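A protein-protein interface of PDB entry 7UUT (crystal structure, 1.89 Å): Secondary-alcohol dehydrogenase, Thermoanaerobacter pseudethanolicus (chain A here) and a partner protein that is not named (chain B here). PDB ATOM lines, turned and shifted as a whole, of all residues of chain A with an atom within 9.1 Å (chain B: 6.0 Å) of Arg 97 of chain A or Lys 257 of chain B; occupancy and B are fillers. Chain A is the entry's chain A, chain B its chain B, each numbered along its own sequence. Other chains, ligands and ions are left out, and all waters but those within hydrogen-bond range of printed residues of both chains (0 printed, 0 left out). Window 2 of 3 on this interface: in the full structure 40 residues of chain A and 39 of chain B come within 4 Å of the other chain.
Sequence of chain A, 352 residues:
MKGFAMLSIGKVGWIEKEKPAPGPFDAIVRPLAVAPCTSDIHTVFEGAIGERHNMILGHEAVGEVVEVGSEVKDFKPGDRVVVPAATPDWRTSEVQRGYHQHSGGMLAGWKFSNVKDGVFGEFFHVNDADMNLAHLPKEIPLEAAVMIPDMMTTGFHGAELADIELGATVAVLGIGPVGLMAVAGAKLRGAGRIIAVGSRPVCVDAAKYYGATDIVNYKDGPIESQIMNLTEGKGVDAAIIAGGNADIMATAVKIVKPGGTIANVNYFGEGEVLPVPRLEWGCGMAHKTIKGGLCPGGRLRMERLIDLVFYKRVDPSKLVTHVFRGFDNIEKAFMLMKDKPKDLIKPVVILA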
ATOM      1  N   TRP A  90      -7.086  34.852 -30.269  1.00  0.00           N
ATOM      2  CA  TRP A  90      -6.396  33.569 -30.322  1.00  0.00           C
ATOM      3  C   TRP A  90      -5.802  33.145 -28.985  1.00  0.00           C
ATOM      4  O   TRP A  90      -5.037  32.175 -28.945  1.00  0.00           O
ATOM      5  CB  TRP A  90      -5.299  33.600 -31.389  1.00  0.00           C
ATOM      6  CG  TRP A  90      -5.847  33.539 -32.774  1.00  0.00           C
ATOM      7  CD1 TRP A  90      -6.063  34.586 -33.622  1.00  0.00           C
ATOM      8  CD2 TRP A  90      -6.294  32.365 -33.462  1.00  0.00           C
ATOM      9  NE1 TRP A  90      -6.598  34.134 -34.804  1.00  0.00           N
ATOM     10  CE2 TRP A  90      -6.752  32.774 -34.730  1.00  0.00           C
ATOM     11  CE3 TRP A  90      -6.346  31.007 -33.130  1.00  0.00           C
ATOM     12  CZ2 TRP A  90      -7.252  31.873 -35.668  1.00  0.00           C
ATOM     13  CZ3 TRP A  90      -6.844  30.114 -34.063  1.00  0.00           C
ATOM     14  CH2 TRP A  90      -7.290  30.551 -35.316  1.00  0.00           C
ATOM     15  N   THR A  92      -7.521  32.277 -25.785  1.00  0.00           N
ATOM     16  CA  THR A  92      -8.595  31.878 -24.885  1.00  0.00           C
ATOM     17  C   THR A  92      -8.587  30.358 -24.768  1.00  0.00           C
ATOM     18  O   THR A  92      -7.841  29.666 -25.465  1.00  0.00           O
ATOM     19  CB  THR A  92      -9.972  32.355 -25.371  1.00  0.00           C
ATOM     20  OG1 THR A  92     -10.243  31.798 -26.663  1.00  0.00           O
ATOM     21  CG2 THR A  92     -10.032  33.877 -25.451  1.00  0.00           C
ATOM     22  N   SER A  93      -9.434  29.837 -23.875  1.00  0.00           N
ATOM     23  CA  SER A  93      -9.526  28.388 -23.711  1.00  0.00           C
ATOM     24  C   SER A  93     -10.205  27.722 -24.901  1.00  0.00           C
ATOM     25  O   SER A  93      -9.837  26.602 -25.272  1.00  0.00           O
ATOM     26  CB  SER A  93     -10.271  28.046 -22.421  1.00  0.00           C
ATOM     27  OG  SER A  93     -11.600  28.539 -22.444  1.00  0.00           O
ATOM     28  N   GLU A  94     -11.197  28.382 -25.509  1.00  0.00           N
ATOM     29  CA  GLU A  94     -11.894  27.797 -26.649  1.00  0.00           C
ATOM     30  C   GLU A  94     -10.979  27.603 -27.851  1.00  0.00           C
ATOM     31  O   GLU A  94     -11.255  26.742 -28.695  1.00  0.00           O
ATOM     32  CB  GLU A  94     -13.094  28.660 -27.050  1.00  0.00           C
ATOM     33  CG  GLU A  94     -14.224  28.685 -26.030  1.00  0.00           C
ATOM     34  CD  GLU A  94     -14.053  29.771 -24.984  1.00  0.00           C
ATOM     35  OE1 GLU A  94     -12.955  30.363 -24.906  1.00  0.00           O
ATOM     36  OE2 GLU A  94     -15.023  30.039 -24.241  1.00  0.00           O
ATOM     37  N   VAL A  95      -9.905  28.388 -27.955  1.00  0.00           N
ATOM     38  CA  VAL A  95      -8.931  28.174 -29.021  1.00  0.00           C
ATOM     39  C   VAL A  95      -8.136  26.901 -28.761  1.00  0.00           C
ATOM     40  O   VAL A  95      -7.827  26.144 -29.688  1.00  0.00           O
ATOM     41  CB  VAL A  95      -8.016  29.403 -29.158  1.00  0.00           C
ATOM     42  CG1 VAL A  95      -6.836  29.099 -30.071  1.00  0.00           C
ATOM     43  CG2 VAL A  95      -8.807  30.584 -29.685  1.00  0.00           C
ATOM     44  N   GLN A  96      -7.804  26.638 -27.494  1.00  0.00           N
ATOM     45  CA  GLN A  96      -7.109  25.405 -27.149  1.00  0.00           C
ATOM     46  C   GLN A  96      -7.984  24.173 -27.347  1.00  0.00           C
ATOM     47  O   GLN A  96      -7.449  23.069 -27.483  1.00  0.00           O
ATOM     48  CB  GLN A  96      -6.605  25.474 -25.704  1.00  0.00           C
ATOM     49  CG  GLN A  96      -5.698  26.664 -25.421  1.00  0.00           C
ATOM     50  CD  GLN A  96      -4.943  26.541 -24.104  1.00  0.00           C
ATOM     51  OE1 GLN A  96      -4.724  25.442 -23.597  1.00  0.00           O
ATOM     52  NE2 GLN A  96      -4.535  27.674 -23.549  1.00  0.00           N
ATOM     53  N   ARG A  97      -9.310  24.336 -27.382  1.00  0.00           N
ATOM     54  CA  ARG A  97     -10.216  23.233 -27.693  1.00  0.00           C
ATOM     55  C   ARG A  97     -10.382  23.003 -29.188  1.00  0.00           C
ATOM     56  O   ARG A  97     -10.965  21.987 -29.578  1.00  0.00           O
ATOM     57  CB  ARG A  97     -11.598  23.480 -27.076  1.00  0.00           C
ATOM     58  CG  ARG A  97     -11.679  23.234 -25.579  1.00  0.00           C
ATOM     59  CD  ARG A  97     -13.117  23.098 -25.092  1.00  0.00           C
ATOM     60  NE  ARG A  97     -13.904  24.306 -25.314  1.00  0.00           N
ATOM     61  CZ  ARG A  97     -14.921  24.392 -26.161  1.00  0.00           C
ATOM     62  NH1 ARG A  97     -15.310  23.351 -26.883  1.00  0.00           N
ATOM     63  NH2 ARG A  97     -15.568  25.548 -26.286  1.00  0.00           N
ATOM     64  N   GLY A  98      -9.893  23.911 -30.029  1.00  0.00           N
ATOM     65  CA  GLY A  98      -9.997  23.748 -31.465  1.00  0.00           C
ATOM     66  C   GLY A  98     -11.201  24.392 -32.114  1.00  0.00           C
ATOM     67  O   GLY A  98     -11.573  23.991 -33.223  1.00  0.00           O
ATOM     68  N   TYR A  99     -11.829  25.375 -31.459  1.00  0.00           N
ATOM     69  CA  TYR A  99     -12.999  26.082 -31.993  1.00  0.00           C
ATOM     70  C   TYR A  99     -12.756  27.581 -31.840  1.00  0.00           C
ATOM     71  O   TYR A  99     -13.319  28.226 -30.953  1.00  0.00           O
ATOM     72  CB  TYR A  99     -14.288  25.632 -31.303  1.00  0.00           C
ATOM     73  CG  TYR A  99     -14.713  24.245 -31.709  1.00  0.00           C
ATOM     74  CD1 TYR A  99     -15.436  24.041 -32.877  1.00  0.00           C
ATOM     75  CD2 TYR A  99     -14.375  23.137 -30.944  1.00  0.00           C
ATOM     76  CE1 TYR A  99     -15.821  22.774 -33.268  1.00  0.00           C
ATOM     77  CE2 TYR A  99     -14.757  21.863 -31.327  1.00  0.00           C
ATOM     78  CZ  TYR A  99     -15.480  21.689 -32.491  1.00  0.00           C
ATOM     79  OH  TYR A  99     -15.867  20.427 -32.884  1.00  0.00           O
ATOM     80  N   HIS A 100     -11.907  28.127 -32.715  1.00  0.00           N
ATOM     81  CA  HIS A 100     -11.607  29.555 -32.662  1.00  0.00           C
ATOM     82  C   HIS A 100     -12.828  30.405 -33.000  1.00  0.00           C
ATOM     83  O   HIS A 100     -12.911  31.560 -32.565  1.00  0.00           O
ATOM     84  CB  HIS A 100     -10.438  29.884 -33.596  1.00  0.00           C
ATOM     85  CG  HIS A 100     -10.726  29.635 -35.046  1.00  0.00           C
ATOM     86  ND1 HIS A 100     -10.307  28.499 -35.704  1.00  0.00           N
ATOM     87  CD2 HIS A 100     -11.375  30.385 -35.968  1.00  0.00           C
ATOM     88  CE1 HIS A 100     -10.694  28.554 -36.966  1.00  0.00           C
ATOM     89  NE2 HIS A 100     -11.345  29.689 -37.152  1.00  0.00           N
ATOM     90  N   GLN A 101     -13.780  29.862 -33.768  1.00  0.00           N
ATOM     91  CA  GLN A 101     -15.000  30.605 -34.067  1.00  0.00           C
ATOM     92  C   GLN A 101     -15.761  30.996 -32.807  1.00  0.00           C
ATOM     93  O   GLN A 101     -16.515  31.976 -32.829  1.00  0.00           O
ATOM     94  CB  GLN A 101     -15.922  29.788 -34.978  1.00  0.00           C
ATOM     95  CG  GLN A 101     -15.321  29.411 -36.319  1.00  0.00           C
ATOM     96  CD  GLN A 101     -14.741  28.015 -36.322  1.00  0.00           C
ATOM     97  OE1 GLN A 101     -14.043  27.620 -35.387  1.00  0.00           O
ATOM     98  NE2 GLN A 101     -15.030  27.255 -37.373  1.00  0.00           N
ATOM     99  N   HIS A 102     -15.569  30.265 -31.710  1.00  0.00           N
ATOM    100  CA  HIS A 102     -16.257  30.535 -30.455  1.00  0.00           C
ATOM    101  C   HIS A 102     -15.281  30.954 -29.365  1.00  0.00           C
ATOM    102  O   HIS A 102     -15.525  30.724 -28.179  1.00  0.00           O
ATOM    103  CB  HIS A 102     -17.067  29.317 -30.016  1.00  0.00           C
ATOM    104  CG  HIS A 102     -17.916  28.745 -31.104  1.00  0.00           C
ATOM    105  ND1 HIS A 102     -19.039  29.384 -31.581  1.00  0.00           N
ATOM    106  CD2 HIS A 102     -17.799  27.602 -31.821  1.00  0.00           C
ATOM    107  CE1 HIS A 102     -19.582  28.658 -32.541  1.00  0.00           C
ATOM    108  NE2 HIS A 102     -18.850  27.570 -32.705  1.00  0.00           N
ATOM    109  N   SER A 103     -14.170  31.570 -29.762  1.00  0.00           N
ATOM    110  CA  SER A 103     -13.160  32.041 -28.823  1.00  0.00           C
ATOM    111  C   SER A 103     -13.725  33.194 -28.003  1.00  0.00           C
ATOM    112  O   SER A 103     -13.884  34.308 -28.512  1.00  0.00           O
ATOM    113  CB  SER A 103     -11.909  32.474 -29.580  1.00  0.00           C
ATOM    114  OG  SER A 103     -10.921  32.971 -28.697  1.00  0.00           O
ATOM    115  N   GLY A 104     -14.026  32.934 -26.731  1.00  0.00           N
ATOM    116  CA  GLY A 104     -14.589  33.946 -25.862  1.00  0.00           C
ATOM    117  C   GLY A 104     -16.098  33.976 -25.788  1.00  0.00           C
ATOM    118  O   GLY A 104     -16.655  34.934 -25.239  1.00  0.00           O
ATOM    119  N   GLY A 105     -16.779  32.964 -26.321  1.00  0.00           N
ATOM    120  CA  GLY A 105     -18.229  32.923 -26.317  1.00  0.00           C
ATOM    121  C   GLY A 105     -18.798  32.397 -27.619  1.00  0.00           C
ATOM    122  O   GLY A 105     -18.076  32.285 -28.613  1.00  0.00           O
ATOM    123  N   MET A 106     -20.089  32.071 -27.628  1.00  0.00           N
ATOM    124  CA  MET A 106     -20.718  31.536 -28.829  1.00  0.00           C
ATOM    125  C   MET A 106     -20.669  32.555 -29.961  1.00  0.00           C
ATOM    126  O   MET A 106     -21.116  33.696 -29.804  1.00  0.00           O
ATOM    127  CB  MET A 106     -22.164  31.143 -28.528  1.00  0.00           C
ATOM    128  CG  MET A 106     -22.810  30.279 -29.596  1.00  0.00           C
ATOM    129  SD  MET A 106     -24.406  29.641 -29.059  1.00  0.00           S
ATOM    130  CE  MET A 106     -23.949  28.788 -27.550  1.00  0.00           C
ATOM    131  N   GLU B 165     -13.172  13.910 -24.459  1.00  0.00           N
ATOM    132  CA  GLU B 165     -11.734  14.056 -24.308  1.00  0.00           C
ATOM    133  C   GLU B 165     -11.345  13.847 -22.846  1.00  0.00           C
ATOM    134  O   GLU B 165     -12.165  13.993 -21.936  1.00  0.00           O
ATOM    135  CB  GLU B 165     -11.279  15.434 -24.794  1.00  0.00           C
ATOM    136  CG  GLU B 165     -11.488  15.663 -26.284  1.00  0.00           C
ATOM    137  CD  GLU B 165     -11.467  17.132 -26.663  1.00  0.00           C
ATOM    138  OE1 GLU B 165     -11.383  17.983 -25.754  1.00  0.00           O
ATOM    139  OE2 GLU B 165     -11.540  17.437 -27.873  1.00  0.00           O
ATOM    140  N   THR B 169     -15.920  17.406 -19.013  1.00  0.00           N
ATOM    141  CA  THR B 169     -17.112  17.365 -18.175  1.00  0.00           C
ATOM    142  C   THR B 169     -18.295  16.863 -18.994  1.00  0.00           C
ATOM    143  O   THR B 169     -18.617  17.431 -20.045  1.00  0.00           O
ATOM    144  CB  THR B 169     -17.415  18.744 -17.590  1.00  0.00           C
ATOM    145  OG1 THR B 169     -16.341  19.135 -16.726  1.00  0.00           O
ATOM    146  CG2 THR B 169     -18.705  18.707 -16.790  1.00  0.00           C
ATOM    147  N   LYS B 234     -20.057  27.769 -17.678  1.00  0.00           N
ATOM    148  CA  LYS B 234     -19.291  27.220 -18.792  1.00  0.00           C
ATOM    149  C   LYS B 234     -20.075  26.182 -19.580  1.00  0.00           C
ATOM    150  O   LYS B 234     -19.853  26.034 -20.788  1.00  0.00           O
ATOM    151  CB  LYS B 234     -17.988  26.600 -18.281  1.00  0.00           C
ATOM    152  CG  LYS B 234     -16.980  27.608 -17.747  1.00  0.00           C
ATOM    153  CD  LYS B 234     -15.661  26.941 -17.364  1.00  0.00           C
ATOM    154  CE  LYS B 234     -15.634  26.533 -15.894  1.00  0.00           C
ATOM    155  NZ  LYS B 234     -16.534  25.385 -15.592  1.00  0.00           N
ATOM    156  N   GLY B 235     -20.992  25.470 -18.933  1.00  0.00           N
ATOM    157  CA  GLY B 235     -21.644  24.346 -19.565  1.00  0.00           C
ATOM    158  C   GLY B 235     -20.786  23.095 -19.501  1.00  0.00           C
ATOM    159  O   GLY B 235     -19.759  23.037 -18.821  1.00  0.00           O
ATOM    160  N   VAL B 236     -21.226  22.074 -20.228  1.00  0.00           N
ATOM    161  CA  VAL B 236     -20.539  20.791 -20.253  1.00  0.00           C
ATOM    162  C   VAL B 236     -19.911  20.585 -21.625  1.00  0.00           C
ATOM    163  O   VAL B 236     -20.314  21.189 -22.625  1.00  0.00           O
ATOM    164  CB  VAL B 236     -21.480  19.620 -19.901  1.00  0.00           C
ATOM    165  CG1 VAL B 236     -22.074  19.817 -18.513  1.00  0.00           C
ATOM    166  CG2 VAL B 236     -22.574  19.482 -20.944  1.00  0.00           C
ATOM    167  N   ASP B 237     -18.887  19.728 -21.658  1.00  0.00           N
ATOM    168  CA  ASP B 237     -18.230  19.386 -22.915  1.00  0.00           C
ATOM    169  C   ASP B 237     -19.064  18.429 -23.756  1.00  0.00           C
ATOM    170  O   ASP B 237     -18.973  18.456 -24.988  1.00  0.00           O
ATOM    171  CB  ASP B 237     -16.852  18.778 -22.640  1.00  0.00           C
ATOM    172  CG  ASP B 237     -15.919  19.744 -21.937  1.00  0.00           C
ATOM    173  OD1 ASP B 237     -15.511  20.741 -22.572  1.00  0.00           O
ATOM    174  OD2 ASP B 237     -15.605  19.519 -20.747  1.00  0.00           O
ATOM    175  N   VAL B 253     -29.032  20.780 -25.651  1.00  0.00           N
ATOM    176  CA  VAL B 253     -28.380  21.826 -26.432  1.00  0.00           C
ATOM    177  C   VAL B 253     -28.038  23.017 -25.545  1.00  0.00           C
ATOM    178  O   VAL B 253     -26.992  23.657 -25.712  1.00  0.00           O
ATOM    179  CB  VAL B 253     -29.273  22.232 -27.620  1.00  0.00           C
ATOM    180  CG1 VAL B 253     -28.680  23.415 -28.363  1.00  0.00           C
ATOM    181  CG2 VAL B 253     -29.472  21.047 -28.560  1.00  0.00           C
ATOM    182  N   LYS B 254     -28.898  23.313 -24.566  1.00  0.00           N
ATOM    183  CA  LYS B 254     -28.695  24.486 -23.724  1.00  0.00           C
ATOM    184  C   LYS B 254     -27.503  24.321 -22.787  1.00  0.00           C
ATOM    185  O   LYS B 254     -26.853  25.313 -22.438  1.00  0.00           O
ATOM    186  CB  LYS B 254     -29.958  24.773 -22.910  1.00  0.00           C
ATOM    187  CG  LYS B 254     -31.163  25.211 -23.727  1.00  0.00           C
ATOM    188  CD  LYS B 254     -32.403  25.306 -22.846  1.00  0.00           C
ATOM    189  CE  LYS B 254     -33.650  25.654 -23.641  1.00  0.00           C
ATOM    190  NZ  LYS B 254     -34.863  25.694 -22.767  1.00  0.00           N
ATOM    191  N   ILE B 255     -27.203  23.093 -22.359  1.00  0.00           N
ATOM    192  CA  ILE B 255     -26.137  22.890 -21.382  1.00  0.00           C
ATOM    193  C   ILE B 255     -24.785  22.568 -22.011  1.00  0.00           C
ATOM    194  O   ILE B 255     -23.754  22.689 -21.332  1.00  0.00           O
ATOM    195  CB  ILE B 255     -26.518  21.784 -20.381  1.00  0.00           C
ATOM    196  CG1 ILE B 255     -26.613  20.430 -21.084  1.00  0.00           C
ATOM    197  CG2 ILE B 255     -27.834  22.118 -19.692  1.00  0.00           C
ATOM    198  CD1 ILE B 255     -26.906  19.287 -20.145  1.00  0.00           C
ATOM    199  N   VAL B 256     -24.751  22.162 -23.273  1.00  0.00           N
ATOM    200  CA  VAL B 256     -23.487  21.861 -23.932  1.00  0.00           C
ATOM    201  C   VAL B 256     -22.855  23.154 -24.415  1.00  0.00           C
ATOM    202  O   VAL B 256     -23.535  24.031 -24.959  1.00  0.00           O
ATOM    203  CB  VAL B 256     -23.705  20.869 -25.086  1.00  0.00           C
ATOM    204  CG1 VAL B 256     -22.447  20.725 -25.916  1.00  0.00           C
ATOM    205  CG2 VAL B 256     -24.095  19.527 -24.532  1.00  0.00           C
ATOM    206  N   LYS B 257     -21.548  23.284 -24.207  1.00  0.00           N
ATOM    207  CA  LYS B 257     -20.829  24.468 -24.640  1.00  0.00           C
ATOM    208  C   LYS B 257     -20.621  24.448 -26.154  1.00  0.00           C
ATOM    209  O   LYS B 257     -20.713  23.394 -26.788  1.00  0.00           O
ATOM    210  CB  LYS B 257     -19.485  24.556 -23.921  1.00  0.00           C
ATOM    211  CG  LYS B 257     -18.538  23.416 -24.233  1.00  0.00           C
ATOM    212  CD  LYS B 257     -17.260  23.537 -23.420  1.00  0.00           C
ATOM    213  CE  LYS B 257     -17.547  23.535 -21.924  1.00  0.00           C
ATOM    214  NZ  LYS B 257     -16.296  23.424 -21.121  1.00  0.00           N
ATOM    215  N   PRO B 258     -20.359  25.609 -26.756  1.00  0.00           N
ATOM    216  CA  PRO B 258     -20.053  25.637 -28.192  1.00  0.00           C
ATOM    217  C   PRO B 258     -18.883  24.720 -28.513  1.00  0.00           C
ATOM    218  O   PRO B 258     -17.866  24.715 -27.817  1.00  0.00           O
ATOM    219  CB  PRO B 258     -19.707  27.108 -28.449  1.00  0.00           C
ATOM    220  CG  PRO B 258     -20.460  27.853 -27.403  1.00  0.00           C
ATOM    221  CD  PRO B 258     -20.453  26.967 -26.187  1.00  0.00           C
ATOM    222  N   GLY B 259     -19.042  23.930 -29.573  1.00  0.00           N
ATOM    223  CA  GLY B 259     -18.062  22.939 -29.949  1.00  0.00           C
ATOM    224  C   GLY B 259     -18.258  21.576 -29.320  1.00  0.00           C
ATOM    225  O   GLY B 259     -17.566  20.626 -29.710  1.00  0.00           O
ATOM    226  N   GLY B 260     -19.173  21.445 -28.365  1.00  0.00           N
ATOM    227  CA  GLY B 260     -19.421  20.175 -27.719  1.00  0.00           C
ATOM    228  C   GLY B 260     -20.316  19.281 -28.555  1.00  0.00           C
ATOM    229  O   GLY B 260     -20.669  19.585 -29.696  1.00  0.00           O
ATOM    230  N   THR B 261     -20.696  18.154 -27.959  1.00  0.00           N
ATOM    231  CA  THR B 261     -21.471  17.134 -28.649  1.00  0.00           C
ATOM    232  C   THR B 261     -22.656  16.706 -27.797  1.00  0.00           C
ATOM    233  O   THR B 261     -22.524  16.497 -26.588  1.00  0.00           O
ATOM    234  CB  THR B 261     -20.602  15.911 -28.988  1.00  0.00           C
ATOM    235  OG1 THR B 261     -19.478  16.326 -29.770  1.00  0.00           O
ATOM    236  CG2 THR B 261     -21.401  14.879 -29.775  1.00  0.00           C
ATOM    237  N   ALA B 286     -23.260  26.998 -33.723  1.00  0.00           N
ATOM    238  CA  ALA B 286     -22.578  26.857 -32.442  1.00  0.00           C
ATOM    239  C   ALA B 286     -21.627  25.670 -32.392  1.00  0.00           C
ATOM    240  O   ALA B 286     -21.030  25.423 -31.337  1.00  0.00           O
ATOM    241  CB  ALA B 286     -23.599  26.732 -31.306  1.00  0.00           C
ATOM    242  N   HIS B 287     -21.469  24.935 -33.495  1.00  0.00           N
ATOM    243  CA  HIS B 287     -20.649  23.722 -33.524  1.00  0.00           C
ATOM    244  C   HIS B 287     -21.084  22.727 -32.450  1.00  0.00           C
ATOM    245  O   HIS B 287     -20.270  21.973 -31.915  1.00  0.00           O
ATOM    246  CB  HIS B 287     -19.159  24.048 -33.391  1.00  0.00           C
ATOM    247  CG  HIS B 287     -18.529  24.538 -34.659  1.00  0.00           C
ATOM    248  ND1 HIS B 287     -18.452  25.876 -34.986  1.00  0.00           N
ATOM    249  CD2 HIS B 287     -17.930  23.869 -35.673  1.00  0.00           C
ATOM    250  CE1 HIS B 287     -17.837  26.009 -36.149  1.00  0.00           C
ATOM    251  NE2 HIS B 287     -17.514  24.805 -36.588  1.00  0.00           N
ATOM    252  N   LYS B 288     -22.375  22.718 -32.121  1.00  0.00           N
ATOM    253  CA  LYS B 288     -22.926  21.738 -31.188  1.00  0.00           C
ATOM    254  C   LYS B 288     -23.429  20.556 -32.005  1.00  0.00           C
ATOM    255  O   LYS B 288     -24.542  20.578 -32.533  1.00  0.00           O
ATOM    256  CB  LYS B 288     -24.033  22.347 -30.337  1.00  0.00           C
ATOM    257  CG  LYS B 288     -23.557  23.455 -29.421  1.00  0.00           C
ATOM    258  CD  LYS B 288     -24.654  23.908 -28.482  1.00  0.00           C
ATOM    259  CE  LYS B 288     -24.230  25.151 -27.727  1.00  0.00           C
ATOM    260  NZ  LYS B 288     -25.274  25.596 -26.770  1.00  0.00           N
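The guanidinium group (NH2) of Arg 97 of chain A sits at hydrogen-bond distance from the backbone carbonyl oxygen (O) of Pro 258 of chain B, at 2.9 Å. A ring nitrogen (NE2) of His 102 of chain A sits at hydrogen-bond distance from the backbone carbonyl oxygen (O) of Ala 286 of chain B, 3.4 Å away. NE2 of His 102 of chain A lies within hydrogen-bond range of ND1 of His 287 of chain B.
The backbone NH of Tyr 99 of chain A is in hydrogen-bond range of the backbone carbonyl oxygen of Glu 94 of chain A (3.1 Å). The backbone carbonyl oxygen (O) of Val 236 of chain B lies within hydrogen-bond range of the backbone NH (N) of Lys 257 of chain B. NZ of Lys 257 of chain B lies within salt-bridge range of OD1 of Asp 237 of chain B (3.1 Å). The side-chain amino group of Lys 288 of chain B sits at hydrogen-bond distance from the backbone carbonyl oxygen of Val 253 of chain B, at 2.8 Å. The backbone NH (N) of Gly 259 of chain B sits at hydrogen-bond distance from the backbone carbonyl oxygen (O) of Ala 286 of chain B, 3.0 Å away. N of Gly 259 of chain B lies close to O of His 287 of chain B (3.3 Å).
Among the printed residues, pairs that only touch across the chains: Gln 101 of chain A with His 287 of chain B (3.3 Å), Tyr 99 of chain A with His 287 of chain B (3.4 Å), Tyr 99 of chain A with Gly 259 of chain B (3.5 Å), Met 106 of chain A with Lys 288 of chain B (3.5 Å), His 102 of chain A with Pro 258 of chain B (3.6 Å), Met 106 of chain A with Pro 258 of chain B (3.6 Å), Arg 97 of chain A with Lys 257 of chain B (3.7 Å) and Met 106 of chain A with Ala 286 of chain B (3.8 Å).
Arg 97 of chain A touches just these residues of chain B: Lys 257 (3.7 Å) and Pro 258 (2.9 Å). Lys 257 of chain B touches just one residue of chain A: Arg 97 (3.7 Å). No residue of chain A comes within 4 Å of Gly 235 of chain B. Asp 237 of chain B touches none of the printed residues of chain A. No residue of chain A comes within 4 Å of Val 256 of chain B. Of chain A, only Arg 97 (2.9 Å), His 102 (3.6 Å) and Met 106 (3.6 Å) come within 4 Å of Pro 258 of chain B. Gly 259 of chain B touches just one residue of chain A: Tyr 99. No residue of chain A comes within 4 Å of Gly 260 of chain B. Printed residues of chain B within 4 Å of Gln 101 of chain A: His 287 (3.3 Å). Printed residues of chain A within 4 Å of His 287 of chain B: Tyr 99 (3.4 Å), Gln 101 (3.3 Å) and His 102 (2.9 Å). Printed residues of chain B within 4 Å of Met 106 of chain A: Pro 258, Ala 286 and Lys 288. Of the printed residues of chain B, His 102 of chain A touches Pro 258 (3.6 Å), Ala 286 (3.4 Å) and His 287 (2.9 Å). The nearest residue of chain B that does not touch Arg 97 of chain A is Gly 259 of chain B (4.1 Å). The nearest residue of chain A that does not touch Lys 257 of chain B is Met 106 of chain A (5.6 Å).
Printed residues of chain B that touch a printed residue of chain A: Lys 257, Pro 258, Gly 259, Ala 286, His 287 and Lys 288. Among the printed residues, 11 pairs touch across the chains. Among the printed residues, no Asp or Glu carboxylate lies within 4 Å of a Lys or Arg side-chain nitrogen of the other chain.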
